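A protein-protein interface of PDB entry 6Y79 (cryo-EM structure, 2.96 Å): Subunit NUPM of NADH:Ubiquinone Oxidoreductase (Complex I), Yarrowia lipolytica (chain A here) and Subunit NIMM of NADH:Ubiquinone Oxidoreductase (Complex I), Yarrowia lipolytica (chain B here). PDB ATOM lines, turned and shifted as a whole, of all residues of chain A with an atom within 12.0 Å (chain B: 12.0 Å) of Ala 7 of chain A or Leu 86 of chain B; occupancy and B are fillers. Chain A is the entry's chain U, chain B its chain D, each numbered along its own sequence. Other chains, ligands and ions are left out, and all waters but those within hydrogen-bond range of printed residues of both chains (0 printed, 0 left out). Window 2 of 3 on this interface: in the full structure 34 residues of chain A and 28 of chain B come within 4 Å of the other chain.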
ATOM      1  N   ARG A   3      31.885 -17.593 -23.130  1.00  0.00           N
ATOM      2  CA  ARG A   3      30.992 -18.463 -23.871  1.00  0.00           C
ATOM      3  C   ARG A   3      30.761 -17.847 -25.242  1.00  0.00           C
ATOM      4  O   ARG A   3      30.897 -16.633 -25.421  1.00  0.00           O
ATOM      5  CB  ARG A   3      29.662 -18.643 -23.137  1.00  0.00           C
ATOM      6  CG  ARG A   3      28.934 -17.337 -22.874  1.00  0.00           C
ATOM      7  CD  ARG A   3      27.590 -17.584 -22.235  1.00  0.00           C
ATOM      8  NE  ARG A   3      26.791 -18.507 -23.032  1.00  0.00           N
ATOM      9  CZ  ARG A   3      25.859 -18.136 -23.900  1.00  0.00           C
ATOM     10  NH1 ARG A   3      25.588 -16.856 -24.078  1.00  0.00           N
ATOM     11  NH2 ARG A   3      25.190 -19.051 -24.584  1.00  0.00           N
ATOM     12  N   GLU A   4      30.447 -18.694 -26.217  1.00  0.00           N
ATOM     13  CA  GLU A   4      30.270 -18.230 -27.586  1.00  0.00           C
ATOM     14  C   GLU A   4      28.790 -18.090 -27.921  1.00  0.00           C
ATOM     15  O   GLU A   4      27.941 -18.775 -27.344  1.00  0.00           O
ATOM     16  CB  GLU A   4      30.994 -19.171 -28.570  1.00  0.00           C
ATOM     17  CG  GLU A   4      30.504 -20.603 -28.638  1.00  0.00           C
ATOM     18  CD  GLU A   4      29.444 -20.777 -29.715  1.00  0.00           C
ATOM     19  OE1 GLU A   4      29.433 -19.961 -30.662  1.00  0.00           O
ATOM     20  OE2 GLU A   4      28.629 -21.697 -29.579  1.00  0.00           O
ATOM     21  N   ALA A   5      28.485 -17.169 -28.835  1.00  0.00           N
ATOM     22  CA  ALA A   5      27.097 -16.839 -29.142  1.00  0.00           C
ATOM     23  C   ALA A   5      26.470 -17.892 -30.050  1.00  0.00           C
ATOM     24  O   ALA A   5      27.034 -18.264 -31.080  1.00  0.00           O
ATOM     25  CB  ALA A   5      27.016 -15.463 -29.804  1.00  0.00           C
ATOM     26  N   ALA A   6      25.289 -18.353 -29.670  1.00  0.00           N
ATOM     27  CA  ALA A   6      24.491 -19.285 -30.437  1.00  0.00           C
ATOM     28  C   ALA A   6      23.113 -18.659 -30.592  1.00  0.00           C
ATOM     29  O   ALA A   6      22.865 -17.561 -30.129  1.00  0.00           O
ATOM     30  CB  ALA A   6      24.381 -20.646 -29.745  1.00  0.00           C
ATOM     31  N   ALA A   7      22.241 -19.351 -31.315  1.00  0.00           N
ATOM     32  CA  ALA A   7      20.802 -19.094 -31.389  1.00  0.00           C
ATOM     33  C   ALA A   7      20.505 -17.665 -31.835  1.00  0.00           C
ATOM     34  O   ALA A   7      20.042 -16.876 -31.043  1.00  0.00           O
ATOM     35  CB  ALA A   7      20.121 -19.386 -30.042  1.00  0.00           C
ATOM     36  N   HIS A   8      20.896 -17.353 -33.071  1.00  0.00           N
ATOM     37  CA  HIS A   8      20.605 -16.077 -33.717  1.00  0.00           C
ATOM     38  C   HIS A   8      21.202 -14.888 -32.945  1.00  0.00           C
ATOM     39  O   HIS A   8      20.496 -14.033 -32.404  1.00  0.00           O
ATOM     40  CB  HIS A   8      19.088 -15.925 -33.911  1.00  0.00           C
ATOM     41  CG  HIS A   8      18.684 -14.749 -34.744  1.00  0.00           C
ATOM     42  ND1 HIS A   8      18.290 -13.551 -34.193  1.00  0.00           N
ATOM     43  CD2 HIS A   8      18.617 -14.587 -36.086  1.00  0.00           C
ATOM     44  CE1 HIS A   8      17.991 -12.703 -35.159  1.00  0.00           C
ATOM     45  NE2 HIS A   8      18.184 -13.306 -36.318  1.00  0.00           N
ATOM     46  N   TRP A   9      22.525 -14.850 -32.869  1.00  0.00           N
ATOM     47  CA  TRP A   9      23.201 -13.610 -32.525  1.00  0.00           C
ATOM     48  C   TRP A   9      23.229 -12.715 -33.759  1.00  0.00           C
ATOM     49  O   TRP A   9      23.414 -13.189 -34.881  1.00  0.00           O
ATOM     50  CB  TRP A   9      24.625 -13.895 -32.044  1.00  0.00           C
ATOM     51  CG  TRP A   9      25.499 -14.569 -33.084  1.00  0.00           C
ATOM     52  CD1 TRP A   9      25.570 -15.902 -33.366  1.00  0.00           C
ATOM     53  CD2 TRP A   9      26.398 -13.922 -33.990  1.00  0.00           C
ATOM     54  NE1 TRP A   9      26.462 -16.123 -34.389  1.00  0.00           N
ATOM     55  CE2 TRP A   9      26.983 -14.921 -34.788  1.00  0.00           C
ATOM     56  CE3 TRP A   9      26.761 -12.594 -34.203  1.00  0.00           C
ATOM     57  CZ2 TRP A   9      27.915 -14.630 -35.780  1.00  0.00           C
ATOM     58  CZ3 TRP A   9      27.692 -12.311 -35.177  1.00  0.00           C
ATOM     59  CH2 TRP A   9      28.254 -13.320 -35.959  1.00  0.00           C
ATOM     60  N   VAL A  10      23.033 -11.413 -33.565  1.00  0.00           N
ATOM     61  CA  VAL A  10      23.211 -10.449 -34.645  1.00  0.00           C
ATOM     62  C   VAL A  10      24.285  -9.442 -34.265  1.00  0.00           C
ATOM     63  O   VAL A  10      24.316  -8.956 -33.130  1.00  0.00           O
ATOM     64  CB  VAL A  10      21.909  -9.752 -35.098  1.00  0.00           C
ATOM     65  CG1 VAL A  10      20.912 -10.796 -35.587  1.00  0.00           C
ATOM     66  CG2 VAL A  10      21.262  -8.822 -34.029  1.00  0.00           C
ATOM     67  N   PRO A  11      25.241  -9.167 -35.151  1.00  0.00           N
ATOM     68  CA  PRO A  11      26.381  -8.324 -34.784  1.00  0.00           C
ATOM     69  C   PRO A  11      26.055  -6.845 -34.870  1.00  0.00           C
ATOM     70  O   PRO A  11      25.233  -6.407 -35.678  1.00  0.00           O
ATOM     71  CB  PRO A  11      27.456  -8.721 -35.800  1.00  0.00           C
ATOM     72  CG  PRO A  11      26.725  -9.300 -36.936  1.00  0.00           C
ATOM     73  CD  PRO A  11      25.430  -9.838 -36.450  1.00  0.00           C
ATOM     74  N   LYS B  81      28.336  -9.169 -30.267  1.00  0.00           N
ATOM     75  CA  LYS B  81      27.251 -10.032 -30.706  1.00  0.00           C
ATOM     76  C   LYS B  81      26.139  -9.973 -29.671  1.00  0.00           C
ATOM     77  O   LYS B  81      26.371 -10.263 -28.495  1.00  0.00           O
ATOM     78  CB  LYS B  81      27.749 -11.461 -30.903  1.00  0.00           C
ATOM     79  CG  LYS B  81      29.062 -11.528 -31.654  1.00  0.00           C
ATOM     80  CD  LYS B  81      29.493 -12.950 -31.903  1.00  0.00           C
ATOM     81  CE  LYS B  81      30.537 -13.006 -32.996  1.00  0.00           C
ATOM     82  NZ  LYS B  81      31.084 -14.371 -33.186  1.00  0.00           N
ATOM     83  N   SER B  82      24.948  -9.570 -30.101  1.00  0.00           N
ATOM     84  CA  SER B  82      23.776  -9.505 -29.237  1.00  0.00           C
ATOM     85  C   SER B  82      22.895 -10.711 -29.529  1.00  0.00           C
ATOM     86  O   SER B  82      22.275 -10.796 -30.592  1.00  0.00           O
ATOM     87  CB  SER B  82      23.006  -8.209 -29.448  1.00  0.00           C
ATOM     88  OG  SER B  82      22.419  -8.180 -30.732  1.00  0.00           O
ATOM     89  N   GLU B  83      22.836 -11.626 -28.574  1.00  0.00           N
ATOM     90  CA  GLU B  83      22.091 -12.867 -28.687  1.00  0.00           C
ATOM     91  C   GLU B  83      20.723 -12.727 -28.033  1.00  0.00           C
ATOM     92  O   GLU B  83      20.594 -12.130 -26.967  1.00  0.00           O
ATOM     93  CB  GLU B  83      22.903 -13.990 -28.042  1.00  0.00           C
ATOM     94  CG  GLU B  83      22.170 -15.283 -27.803  1.00  0.00           C
ATOM     95  CD  GLU B  83      23.057 -16.378 -27.293  1.00  0.00           C
ATOM     96  OE1 GLU B  83      24.249 -16.122 -27.020  1.00  0.00           O
ATOM     97  OE2 GLU B  83      22.578 -17.517 -27.202  1.00  0.00           O
ATOM     98  N   ARG B  84      19.709 -13.322 -28.665  1.00  0.00           N
ATOM     99  CA  ARG B  84      18.275 -13.279 -28.389  1.00  0.00           C
ATOM    100  C   ARG B  84      17.908 -13.820 -26.995  1.00  0.00           C
ATOM    101  O   ARG B  84      18.793 -14.363 -26.321  1.00  0.00           O
ATOM    102  CB  ARG B  84      17.607 -14.046 -29.535  1.00  0.00           C
ATOM    103  CG  ARG B  84      17.637 -15.518 -29.405  1.00  0.00           C
ATOM    104  CD  ARG B  84      16.931 -16.096 -30.595  1.00  0.00           C
ATOM    105  NE  ARG B  84      15.531 -15.733 -30.528  1.00  0.00           N
ATOM    106  CZ  ARG B  84      14.614 -16.468 -29.921  1.00  0.00           C
ATOM    107  NH1 ARG B  84      14.951 -17.613 -29.360  1.00  0.00           N
ATOM    108  NH2 ARG B  84      13.362 -16.061 -29.887  1.00  0.00           N
ATOM    109  N   PRO B  85      16.652 -13.662 -26.507  1.00  0.00           N
ATOM    110  CA  PRO B  85      16.349 -14.001 -25.099  1.00  0.00           C
ATOM    111  C   PRO B  85      16.583 -15.433 -24.630  1.00  0.00           C
ATOM    112  O   PRO B  85      16.645 -15.624 -23.410  1.00  0.00           O
ATOM    113  CB  PRO B  85      14.857 -13.671 -24.997  1.00  0.00           C
ATOM    114  CG  PRO B  85      14.704 -12.538 -25.841  1.00  0.00           C
ATOM    115  CD  PRO B  85      15.581 -12.778 -27.023  1.00  0.00           C
ATOM    116  N   LEU B  86      16.682 -16.420 -25.530  1.00  0.00           N
ATOM    117  CA  LEU B  86      16.820 -17.848 -25.200  1.00  0.00           C
ATOM    118  C   LEU B  86      15.636 -18.336 -24.356  1.00  0.00           C
ATOM    119  O   LEU B  86      15.780 -18.794 -23.223  1.00  0.00           O
ATOM    120  CB  LEU B  86      18.165 -18.134 -24.512  1.00  0.00           C
ATOM    121  CG  LEU B  86      18.958 -19.414 -24.757  1.00  0.00           C
ATOM    122  CD1 LEU B  86      19.360 -19.545 -26.190  1.00  0.00           C
ATOM    123  CD2 LEU B  86      20.199 -19.330 -23.952  1.00  0.00           C
ATOM    124  N   ILE B  87      14.453 -18.210 -24.946  1.00  0.00           N
ATOM    125  CA  ILE B  87      13.186 -18.568 -24.337  1.00  0.00           C
ATOM    126  C   ILE B  87      13.068 -20.080 -24.132  1.00  0.00           C
ATOM    127  O   ILE B  87      12.995 -20.577 -23.001  1.00  0.00           O
ATOM    128  CB  ILE B  87      12.033 -18.007 -25.202  1.00  0.00           C
ATOM    129  CG1 ILE B  87      12.186 -16.482 -25.362  1.00  0.00           C
ATOM    130  CG2 ILE B  87      10.680 -18.365 -24.630  1.00  0.00           C
ATOM    131  CD1 ILE B  87      11.132 -15.810 -26.239  1.00  0.00           C
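Of the printed residues of chain B, Ala 7 of chain A touches Arg 84 and Leu 86.
Of chain A, only Ala 7 comes within 4 Å of Leu 86 of chain B.
Of chain B, only Glu 83 comes within 4 Å of Ala 5 of chain A.
Of chain B, only Glu 83 (2.9 Å) comes within 4 Å of Ala 6 of chain A.
Of the printed residues of chain B, His 8 of chain A touches Arg 84 (3.9 Å).
Glu 83 of chain B touches just these residues of chain A: Arg 3, Ala 5 and Ala 6.
Printed residues of chain B within 4 Å of Val 10 of chain A: Lys 81 and Ser 82.
Printed residues of chain A within 4 Å of Ser 82 of chain B: Trp 9 (3.5 Å) and Val 10 (3.1 Å).
Of the printed residues of chain A, Lys 81 of chain B touches Trp 9 and Val 10.
Glu 4 of chain A touches none of the printed residues of chain B.
The nearest residue of chain A that does not touch Leu 86 of chain B is Arg 3 of chain A (5.0 Å).
Printed residues of chain A that touch a printed residue of chain B: Arg 3, Ala 5, Ala 6, Ala 7, His 8, Trp 9 and Val 10.
Hydrophobic or aromatic side chains of chain A that line the printed part of chain B: Ala 5, Ala 7, His 8, Trp 9 and Val 10.
Of the 7 printed residues of chain B, 5 touch a printed residue of chain A.
Among the printed residues, Asp or Glu carboxylates within 4 Å of a Lys or Arg side-chain nitrogen of the other chain: Arg 3 of chain A with Glu 83 of chain B (3.3 Å).
The backbone NH (N) of Val 10 of chain A is in hydrogen-bond range of the backbone carbonyl oxygen (O) of Ser 82 of chain B, at 3.1 Å.
OE2 of Glu 83 of chain B lies close to O of Ala 6 of chain A, at 2.9 Å.
The guanidinium group (NH1) of Arg 3 of chain A is in salt-bridge range of the side-chain carboxylate (OE1) of Glu 83 of chain B.
Among the printed residues, merely in contact across the chains: Ala 7 of chain A with Arg 84 of chain B, Trp 9 of chain A with Ser 82 of chain B, Trp 9 of chain A with Lys 81 of chain B, Ala 5 of chain A with Glu 83 of chain B, His 8 of chain A with Arg 84 of chain B, Ala 7 of chain A with Leu 86 of chain B and Val 10 of chain A with Lys 81 of chain B.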
